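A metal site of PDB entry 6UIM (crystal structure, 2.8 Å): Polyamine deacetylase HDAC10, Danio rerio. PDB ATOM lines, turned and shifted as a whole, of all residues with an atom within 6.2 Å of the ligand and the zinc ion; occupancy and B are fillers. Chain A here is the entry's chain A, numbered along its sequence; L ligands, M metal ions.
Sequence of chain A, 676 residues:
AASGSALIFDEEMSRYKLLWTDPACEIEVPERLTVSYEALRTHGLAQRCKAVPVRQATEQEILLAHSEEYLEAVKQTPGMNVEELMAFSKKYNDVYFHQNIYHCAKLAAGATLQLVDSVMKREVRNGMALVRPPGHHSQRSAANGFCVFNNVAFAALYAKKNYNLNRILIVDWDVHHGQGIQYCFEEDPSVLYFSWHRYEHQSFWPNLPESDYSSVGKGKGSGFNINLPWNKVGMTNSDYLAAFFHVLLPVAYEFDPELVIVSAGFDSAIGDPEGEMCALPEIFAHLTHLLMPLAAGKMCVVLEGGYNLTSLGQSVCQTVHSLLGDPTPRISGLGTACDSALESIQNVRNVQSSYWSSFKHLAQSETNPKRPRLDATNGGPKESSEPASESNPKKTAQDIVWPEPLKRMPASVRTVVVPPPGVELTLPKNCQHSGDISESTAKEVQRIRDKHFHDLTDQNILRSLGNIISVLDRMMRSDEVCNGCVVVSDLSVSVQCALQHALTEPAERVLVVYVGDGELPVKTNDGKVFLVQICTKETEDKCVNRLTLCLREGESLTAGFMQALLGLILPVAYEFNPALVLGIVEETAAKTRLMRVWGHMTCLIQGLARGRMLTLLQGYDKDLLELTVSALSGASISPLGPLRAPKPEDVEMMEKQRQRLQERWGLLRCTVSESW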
ATOM      1  N   ALA A  24     -15.787 -24.125 -26.839  1.00  0.00           N
ATOM      2  CA  ALA A  24     -14.693 -25.018 -26.481  1.00  0.00           C
ATOM      3  C   ALA A  24     -13.864 -25.406 -27.701  1.00  0.00           C
ATOM      4  O   ALA A  24     -12.665 -25.666 -27.568  1.00  0.00           O
ATOM      5  CB  ALA A  24     -15.254 -26.275 -25.804  1.00  0.00           C
ATOM      6  N   CYS A  25     -14.487 -25.427 -28.888  1.00  0.00           N
ATOM      7  CA  CYS A  25     -13.862 -25.923 -30.108  1.00  0.00           C
ATOM      8  C   CYS A  25     -13.444 -24.810 -31.052  1.00  0.00           C
ATOM      9  O   CYS A  25     -12.764 -25.078 -32.053  1.00  0.00           O
ATOM     10  CB  CYS A  25     -14.850 -26.851 -30.835  1.00  0.00           C
ATOM     11  SG  CYS A  25     -15.239 -28.391 -29.977  1.00  0.00           S
ATOM     12  N   ILE A  27     -11.254 -22.644 -31.044  1.00  0.00           N
ATOM     13  CA  ILE A  27      -9.834 -22.415 -31.258  1.00  0.00           C
ATOM     14  C   ILE A  27      -9.255 -23.339 -32.306  1.00  0.00           C
ATOM     15  O   ILE A  27      -8.218 -23.018 -32.911  1.00  0.00           O
ATOM     16  CB  ILE A  27      -9.055 -22.566 -29.935  1.00  0.00           C
ATOM     17  CG1 ILE A  27      -9.244 -23.976 -29.362  1.00  0.00           C
ATOM     18  CG2 ILE A  27      -9.498 -21.509 -28.940  1.00  0.00           C
ATOM     19  CD1 ILE A  27      -8.338 -24.287 -28.193  1.00  0.00           C
ATOM     20  N   ASP A  94     -15.940 -32.344 -26.181  1.00  0.00           N
ATOM     21  CA  ASP A  94     -15.083 -31.318 -26.777  1.00  0.00           C
ATOM     22  C   ASP A  94     -14.546 -31.744 -28.141  1.00  0.00           C
ATOM     23  O   ASP A  94     -13.347 -31.654 -28.418  1.00  0.00           O
ATOM     24  CB  ASP A  94     -13.935 -30.963 -25.833  1.00  0.00           C
ATOM     25  CG  ASP A  94     -14.376 -30.050 -24.720  1.00  0.00           C
ATOM     26  OD1 ASP A  94     -15.518 -29.535 -24.785  1.00  0.00           O
ATOM     27  OD2 ASP A  94     -13.570 -29.835 -23.777  1.00  0.00           O
ATOM     28  N   PRO A 134      -5.851 -33.572 -34.523  1.00  0.00           N
ATOM     29  CA  PRO A 134      -4.818 -34.203 -33.681  1.00  0.00           C
ATOM     30  C   PRO A 134      -5.235 -35.596 -33.260  1.00  0.00           C
ATOM     31  O   PRO A 134      -6.207 -36.140 -33.787  1.00  0.00           O
ATOM     32  CB  PRO A 134      -4.723 -33.258 -32.469  1.00  0.00           C
ATOM     33  CG  PRO A 134      -5.495 -32.019 -32.857  1.00  0.00           C
ATOM     34  CD  PRO A 134      -6.526 -32.482 -33.809  1.00  0.00           C
ATOM     35  N   HIS A 136      -3.855 -37.408 -29.716  1.00  0.00           N
ATOM     36  CA  HIS A 136      -3.510 -38.005 -28.432  1.00  0.00           C
ATOM     37  C   HIS A 136      -4.664 -38.078 -27.440  1.00  0.00           C
ATOM     38  O   HIS A 136      -4.517 -38.716 -26.397  1.00  0.00           O
ATOM     39  CB  HIS A 136      -2.322 -37.265 -27.799  1.00  0.00           C
ATOM     40  CG  HIS A 136      -2.598 -35.831 -27.454  1.00  0.00           C
ATOM     41  ND1 HIS A 136      -1.712 -35.065 -26.721  1.00  0.00           N
ATOM     42  CD2 HIS A 136      -3.636 -35.028 -27.743  1.00  0.00           C
ATOM     43  CE1 HIS A 136      -2.199 -33.845 -26.584  1.00  0.00           C
ATOM     44  NE2 HIS A 136      -3.379 -33.799 -27.189  1.00  0.00           N
ATOM     45  N   HIS A 137      -5.820 -37.472 -27.739  1.00  0.00           N
ATOM     46  CA  HIS A 137      -6.955 -37.594 -26.840  1.00  0.00           C
ATOM     47  C   HIS A 137      -7.950 -38.667 -27.274  1.00  0.00           C
ATOM     48  O   HIS A 137      -8.764 -39.092 -26.444  1.00  0.00           O
ATOM     49  CB  HIS A 137      -7.688 -36.252 -26.729  1.00  0.00           C
ATOM     50  CG  HIS A 137      -6.882 -35.189 -26.084  1.00  0.00           C
ATOM     51  ND1 HIS A 137      -6.301 -35.349 -24.842  1.00  0.00           N
ATOM     52  CD2 HIS A 137      -6.516 -33.952 -26.506  1.00  0.00           C
ATOM     53  CE1 HIS A 137      -5.636 -34.246 -24.524  1.00  0.00           C
ATOM     54  NE2 HIS A 137      -5.749 -33.398 -25.516  1.00  0.00           N
ATOM     55  N   GLY A 145     -11.678 -34.428 -27.377  1.00  0.00           N
ATOM     56  CA  GLY A 145     -10.834 -33.260 -27.405  1.00  0.00           C
ATOM     57  C   GLY A 145     -10.166 -32.965 -28.734  1.00  0.00           C
ATOM     58  O   GLY A 145      -8.942 -33.005 -28.828  1.00  0.00           O
ATOM     59  N   PHE A 146     -10.984 -32.689 -29.769  1.00  0.00           N
ATOM     60  CA  PHE A 146     -10.545 -32.273 -31.097  1.00  0.00           C
ATOM     61  C   PHE A 146     -10.013 -33.425 -31.946  1.00  0.00           C
ATOM     62  O   PHE A 146      -9.818 -33.259 -33.162  1.00  0.00           O
ATOM     63  CB  PHE A 146      -9.463 -31.184 -31.023  1.00  0.00           C
ATOM     64  CG  PHE A 146      -9.879 -29.926 -30.298  1.00  0.00           C
ATOM     65  CD1 PHE A 146     -11.209 -29.663 -29.989  1.00  0.00           C
ATOM     66  CD2 PHE A 146      -8.923 -28.986 -29.952  1.00  0.00           C
ATOM     67  CE1 PHE A 146     -11.564 -28.497 -29.333  1.00  0.00           C
ATOM     68  CE2 PHE A 146      -9.276 -27.808 -29.304  1.00  0.00           C
ATOM     69  CZ  PHE A 146     -10.593 -27.565 -28.997  1.00  0.00           C
ATOM     70  N   CYS A 147      -9.776 -34.586 -31.333  1.00  0.00           N
ATOM     71  CA  CYS A 147      -9.124 -35.716 -31.984  1.00  0.00           C
ATOM     72  C   CYS A 147     -10.116 -36.822 -32.341  1.00  0.00           C
ATOM     73  O   CYS A 147     -10.949 -37.210 -31.512  1.00  0.00           O
ATOM     74  CB  CYS A 147      -8.021 -36.287 -31.104  1.00  0.00           C
ATOM     75  SG  CYS A 147      -7.068 -35.071 -30.191  1.00  0.00           S
ATOM     76  N   ASP A 174       2.541 -31.432 -25.584  1.00  0.00           N
ATOM     77  CA  ASP A 174       1.299 -30.682 -25.477  1.00  0.00           C
ATOM     78  C   ASP A 174       0.977 -30.415 -23.997  1.00  0.00           C
ATOM     79  O   ASP A 174       1.474 -31.094 -23.089  1.00  0.00           O
ATOM     80  CB  ASP A 174       0.180 -31.486 -26.151  1.00  0.00           C
ATOM     81  CG  ASP A 174      -0.992 -30.621 -26.567  1.00  0.00           C
ATOM     82  OD1 ASP A 174      -1.598 -29.958 -25.705  1.00  0.00           O
ATOM     83  OD2 ASP A 174      -1.307 -30.619 -27.782  1.00  0.00           O
ATOM     84  N   VAL A 175       0.162 -29.379 -23.757  1.00  0.00           N
ATOM     85  CA  VAL A 175      -0.279 -29.037 -22.394  1.00  0.00           C
ATOM     86  C   VAL A 175      -1.472 -29.850 -21.925  1.00  0.00           C
ATOM     87  O   VAL A 175      -1.913 -29.689 -20.775  1.00  0.00           O
ATOM     88  CB  VAL A 175      -0.689 -27.563 -22.197  1.00  0.00           C
ATOM     89  CG1 VAL A 175       0.534 -26.687 -21.950  1.00  0.00           C
ATOM     90  CG2 VAL A 175      -1.485 -27.083 -23.384  1.00  0.00           C
ATOM     91  N   HIS A 176      -2.042 -30.686 -22.778  1.00  0.00           N
ATOM     92  CA  HIS A 176      -3.135 -31.565 -22.408  1.00  0.00           C
ATOM     93  C   HIS A 176      -2.614 -32.987 -22.279  1.00  0.00           C
ATOM     94  O   HIS A 176      -1.747 -33.409 -23.047  1.00  0.00           O
ATOM     95  CB  HIS A 176      -4.258 -31.488 -23.435  1.00  0.00           C
ATOM     96  CG  HIS A 176      -4.838 -30.132 -23.598  1.00  0.00           C
ATOM     97  ND1 HIS A 176      -4.308 -29.192 -24.456  1.00  0.00           N
ATOM     98  CD2 HIS A 176      -5.901 -29.544 -23.008  1.00  0.00           C
ATOM     99  CE1 HIS A 176      -5.029 -28.080 -24.387  1.00  0.00           C
ATOM    100  NE2 HIS A 176      -5.999 -28.267 -23.522  1.00  0.00           N
ATOM    101  N   ARG A 198      -0.906 -29.393 -18.370  1.00  0.00           N
ATOM    102  CA  ARG A 198      -1.543 -28.507 -17.404  1.00  0.00           C
ATOM    103  C   ARG A 198      -2.585 -29.282 -16.618  1.00  0.00           C
ATOM    104  O   ARG A 198      -3.511 -29.860 -17.210  1.00  0.00           O
ATOM    105  CB  ARG A 198      -2.157 -27.302 -18.097  1.00  0.00           C
ATOM    106  CG  ARG A 198      -2.860 -26.335 -17.165  1.00  0.00           C
ATOM    107  CD  ARG A 198      -3.516 -25.200 -17.946  1.00  0.00           C
ATOM    108  NE  ARG A 198      -4.379 -24.373 -17.101  1.00  0.00           N
ATOM    109  CZ  ARG A 198      -5.140 -23.383 -17.561  1.00  0.00           C
ATOM    110  NH1 ARG A 198      -5.159 -23.098 -18.852  1.00  0.00           N
ATOM    111  NH2 ARG A 198      -5.888 -22.676 -16.715  1.00  0.00           N
ATOM    112  N   PHE A 204      -8.279 -28.848 -14.358  1.00  0.00           N
ATOM    113  CA  PHE A 204      -8.146 -28.492 -15.766  1.00  0.00           C
ATOM    114  C   PHE A 204      -8.465 -29.684 -16.667  1.00  0.00           C
ATOM    115  O   PHE A 204      -8.266 -30.844 -16.289  1.00  0.00           O
ATOM    116  CB  PHE A 204      -6.738 -27.983 -16.090  1.00  0.00           C
ATOM    117  CG  PHE A 204      -6.621 -27.362 -17.452  1.00  0.00           C
ATOM    118  CD1 PHE A 204      -7.291 -26.184 -17.745  1.00  0.00           C
ATOM    119  CD2 PHE A 204      -5.861 -27.967 -18.437  1.00  0.00           C
ATOM    120  CE1 PHE A 204      -7.190 -25.610 -19.004  1.00  0.00           C
ATOM    121  CE2 PHE A 204      -5.758 -27.406 -19.701  1.00  0.00           C
ATOM    122  CZ  PHE A 204      -6.427 -26.219 -19.979  1.00  0.00           C
ATOM    123  N   TRP A 205      -8.965 -29.365 -17.862  1.00  0.00           N
ATOM    124  CA  TRP A 205      -9.394 -30.375 -18.813  1.00  0.00           C
ATOM    125  C   TRP A 205      -8.216 -31.281 -19.200  1.00  0.00           C
ATOM    126  O   TRP A 205      -7.109 -30.792 -19.443  1.00  0.00           O
ATOM    127  CB  TRP A 205      -9.969 -29.719 -20.061  1.00  0.00           C
ATOM    128  CG  TRP A 205     -10.689 -30.657 -20.958  1.00  0.00           C
ATOM    129  CD1 TRP A 205     -12.028 -30.939 -20.967  1.00  0.00           C
ATOM    130  CD2 TRP A 205     -10.101 -31.483 -21.975  1.00  0.00           C
ATOM    131  NE1 TRP A 205     -12.303 -31.879 -21.922  1.00  0.00           N
ATOM    132  CE2 TRP A 205     -11.144 -32.239 -22.548  1.00  0.00           C
ATOM    133  CE3 TRP A 205      -8.795 -31.667 -22.439  1.00  0.00           C
ATOM    134  CZ2 TRP A 205     -10.922 -33.141 -23.579  1.00  0.00           C
ATOM    135  CZ3 TRP A 205      -8.577 -32.569 -23.456  1.00  0.00           C
ATOM    136  CH2 TRP A 205      -9.641 -33.299 -24.024  1.00  0.00           C
ATOM    137  N   GLY A 265       2.592 -30.747 -29.618  1.00  0.00           N
ATOM    138  CA  GLY A 265       1.560 -29.740 -29.493  1.00  0.00           C
ATOM    139  C   GLY A 265       2.170 -28.441 -29.002  1.00  0.00           C
ATOM    140  O   GLY A 265       2.868 -28.427 -27.985  1.00  0.00           O
ATOM    141  N   ASP A 267       0.555 -25.628 -28.080  1.00  0.00           N
ATOM    142  CA  ASP A 267      -0.226 -24.853 -27.117  1.00  0.00           C
ATOM    143  C   ASP A 267       0.464 -24.761 -25.761  1.00  0.00           C
ATOM    144  O   ASP A 267      -0.101 -24.153 -24.844  1.00  0.00           O
ATOM    145  CB  ASP A 267      -1.628 -25.446 -26.939  1.00  0.00           C
ATOM    146  CG  ASP A 267      -1.609 -26.955 -26.806  1.00  0.00           C
ATOM    147  OD1 ASP A 267      -0.513 -27.535 -26.735  1.00  0.00           O
ATOM    148  OD2 ASP A 267      -2.701 -27.552 -26.756  1.00  0.00           O
ATOM    149  N   PRO A 273      -4.171 -19.482 -25.904  1.00  0.00           N
ATOM    150  CA  PRO A 273      -5.365 -19.213 -25.102  1.00  0.00           C
ATOM    151  C   PRO A 273      -5.817 -20.390 -24.259  1.00  0.00           C
ATOM    152  O   PRO A 273      -6.692 -20.232 -23.411  1.00  0.00           O
ATOM    153  CB  PRO A 273      -6.422 -18.854 -26.158  1.00  0.00           C
ATOM    154  CG  PRO A 273      -5.998 -19.629 -27.362  1.00  0.00           C
ATOM    155  CD  PRO A 273      -4.484 -19.625 -27.342  1.00  0.00           C
ATOM    156  N   GLU A 274      -5.241 -21.574 -24.476  1.00  0.00           N
ATOM    157  CA  GLU A 274      -5.643 -22.782 -23.756  1.00  0.00           C
ATOM    158  C   GLU A 274      -4.626 -23.221 -22.713  1.00  0.00           C
ATOM    159  O   GLU A 274      -5.015 -23.655 -21.628  1.00  0.00           O
ATOM    160  CB  GLU A 274      -5.872 -23.926 -24.746  1.00  0.00           C
ATOM    161  CG  GLU A 274      -6.541 -25.142 -24.157  1.00  0.00           C
ATOM    162  CD  GLU A 274      -8.048 -25.033 -24.162  1.00  0.00           C
ATOM    163  OE1 GLU A 274      -8.689 -25.785 -23.407  1.00  0.00           O
ATOM    164  OE2 GLU A 274      -8.577 -24.196 -24.908  1.00  0.00           O
ATOM    165  N   GLU A 276      -1.905 -21.299 -21.507  1.00  0.00           N
ATOM    166  CA  GLU A 276      -1.549 -20.173 -20.655  1.00  0.00           C
ATOM    167  C   GLU A 276      -0.172 -20.336 -20.025  1.00  0.00           C
ATOM    168  O   GLU A 276       0.062 -19.897 -18.903  1.00  0.00           O
ATOM    169  CB  GLU A 276      -2.604 -19.951 -19.562  1.00  0.00           C
ATOM    170  CG  GLU A 276      -4.003 -19.619 -20.089  1.00  0.00           C
ATOM    171  CD  GLU A 276      -5.020 -19.507 -18.960  1.00  0.00           C
ATOM    172  OE1 GLU A 276      -4.621 -19.675 -17.794  1.00  0.00           O
ATOM    173  OE2 GLU A 276      -6.215 -19.258 -19.247  1.00  0.00           O
ATOM    174  N   GLU A 304       0.213 -31.786 -32.890  1.00  0.00           N
ATOM    175  CA  GLU A 304      -0.895 -32.067 -31.991  1.00  0.00           C
ATOM    176  C   GLU A 304      -1.748 -30.810 -31.827  1.00  0.00           C
ATOM    177  O   GLU A 304      -2.664 -30.578 -32.621  1.00  0.00           O
ATOM    178  CB  GLU A 304      -0.361 -32.576 -30.650  1.00  0.00           C
ATOM    179  CG  GLU A 304      -1.211 -33.637 -29.989  1.00  0.00           C
ATOM    180  CD  GLU A 304      -1.314 -34.928 -30.787  1.00  0.00           C
ATOM    181  OE1 GLU A 304      -2.369 -35.162 -31.396  1.00  0.00           O
ATOM    182  OE2 GLU A 304      -0.328 -35.704 -30.798  1.00  0.00           O
ATOM    183  N   GLY A 305      -1.438 -29.991 -30.828  1.00  0.00           N
ATOM    184  CA  GLY A 305      -2.160 -28.766 -30.569  1.00  0.00           C
ATOM    185  C   GLY A 305      -1.329 -27.521 -30.815  1.00  0.00           C
ATOM    186  O   GLY A 305      -0.201 -27.565 -31.316  1.00  0.00           O
ATOM    187  N   GLY A 306      -1.907 -26.375 -30.439  1.00  0.00           N
ATOM    188  CA  GLY A 306      -1.326 -25.067 -30.685  1.00  0.00           C
ATOM    189  C   GLY A 306      -2.333 -24.161 -31.359  1.00  0.00           C
ATOM    190  O   GLY A 306      -2.735 -24.421 -32.495  1.00  0.00           O
ATOM    191  N   TYR A 307      -2.767 -23.089 -30.681  1.00  0.00           N
ATOM    192  CA  TYR A 307      -3.916 -22.327 -31.155  1.00  0.00           C
ATOM    193  C   TYR A 307      -3.710 -20.826 -31.212  1.00  0.00           C
ATOM    194  O   TYR A 307      -4.668 -20.106 -31.529  1.00  0.00           O
ATOM    195  CB  TYR A 307      -5.142 -22.651 -30.280  1.00  0.00           C
ATOM    196  CG  TYR A 307      -5.375 -24.131 -30.159  1.00  0.00           C
ATOM    197  CD1 TYR A 307      -6.147 -24.807 -31.088  1.00  0.00           C
ATOM    198  CD2 TYR A 307      -4.782 -24.858 -29.137  1.00  0.00           C
ATOM    199  CE1 TYR A 307      -6.351 -26.172 -30.984  1.00  0.00           C
ATOM    200  CE2 TYR A 307      -4.977 -26.218 -29.023  1.00  0.00           C
ATOM    201  CZ  TYR A 307      -5.771 -26.869 -29.946  1.00  0.00           C
ATOM    202  OH  TYR A 307      -5.970 -28.226 -29.840  1.00  0.00           O
HETATM  203  C1  LIG L   1      -8.261 -30.114 -26.575  1.00  0.00           C
HETATM  204  C2  LIG L   1      -6.893 -29.841 -27.128  1.00  0.00           C
HETATM  205  C3  LIG L   1      -6.282 -30.873 -28.023  1.00  0.00           C
HETATM  206  C4  LIG L   1      -9.914 -24.052 -20.699  1.00  0.00           C
HETATM  207  C5  LIG L   1     -11.230 -24.747 -21.093  1.00  0.00           C
HETATM  208  C6  LIG L   1     -10.966 -26.236 -21.407  1.00  0.00           C
HETATM  209  C7  LIG L   1     -10.992 -27.866 -23.315  1.00  0.00           C
HETATM  210  C8  LIG L   1     -10.911 -27.856 -24.848  1.00  0.00           C
HETATM  211  C9  LIG L   1     -10.265 -29.121 -25.408  1.00  0.00           C
HETATM  212  C10 LIG L   1      -8.954 -28.844 -26.119  1.00  0.00           C
HETATM  213  N1  LIG L   1     -10.067 -22.592 -20.794  1.00  0.00           N
HETATM  214  N2  LIG L   1     -11.322 -26.509 -22.817  1.00  0.00           N
HETATM  215  O1  LIG L   1      -6.283 -28.816 -26.872  1.00  0.00           O
HETATM  216  S1  LIG L   1      -4.517 -30.780 -27.869  1.00  0.00           S
HETATM  217 ZN    ZN M   1      -3.412 -29.507 -26.463  1.00  0.00          ZN
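The side-chain carboxylate of Glu 274 is in salt-bridge range of a nitrogen (N2) of the ligand. A sulfur (S1) of the ligand lies close to a ring nitrogen (NE2) of His 136. A ring nitrogen (NE2) of His 137 lies close to a sulfur (S1) of the ligand (3.7 Å). The side-chain hydroxyl (OH) of Tyr 307 lies within hydrogen-bond range of an oxygen (O1) of the ligand (3.0 Å).
O of Asp 94 sits close to N of Gly 145, 3.4 Å away. N of Gly 305 sits at hydrogen-bond distance from OD2 of Asp 174 (3.1 Å). A ring nitrogen (NE2) of His 137 sits at hydrogen-bond distance from a ring nitrogen (NE2) of His 136 (2.9 Å). The backbone NH (N) of His 136 lies within hydrogen-bond range of the side-chain carboxylate (OE1) of Glu 304, 3.2 Å away. The backbone carbonyl oxygen (O) of Gly 145 sits at hydrogen-bond distance from the side-chain sulfur (SG) of Cys 147 (3.1 Å). The guanidinium group of Arg 198 is in hydrogen-bond range of the backbone carbonyl oxygen of Glu 274, 2.8 Å away. The backbone NH of Phe 146 is in hydrogen-bond range of the backbone carbonyl oxygen of Asp 94 (2.9 Å). The indole nitrogen (NE1) of Trp 205 lies within hydrogen-bond range of the side-chain carboxylate (OD2) of Asp 94, 3.0 Å away.
Ala 24 touches the ligand (O to C8, 3.9 Å). Asp 94 touches the ligand (OD2 to C7, 3.3 Å). Gly 145 touches the ligand (O to C3, 3.5 Å). CE2 of Phe 146 touches C10 of the ligand (3.4 Å). Phe 204 touches the ligand. Trp 205 touches the ligand (CG to C7, 3.7 Å). Of the 25 residues printed, 13 come within 4 Å of the ligand. The nearest printed residue that does not touch the ligand is Gly 305 (4.1 Å).
Of the 25 residues printed, 3 come within 4 Å of the zinc ion.
The zinc ion is bound by OD1 of Asp 174 (2.0 Å). The zinc ion is bound by OD2 of Asp 267 (2.1 Å). S1 of the ligand binds the zinc ion, 2.2 Å away. The zinc ion is bound by ND1 of His 176. The zinc ion has four donor atoms within binding distance. Slightly farther from the zinc ion lies the side-chain carboxylate (OD2) of Asp 174 (2.7 Å).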
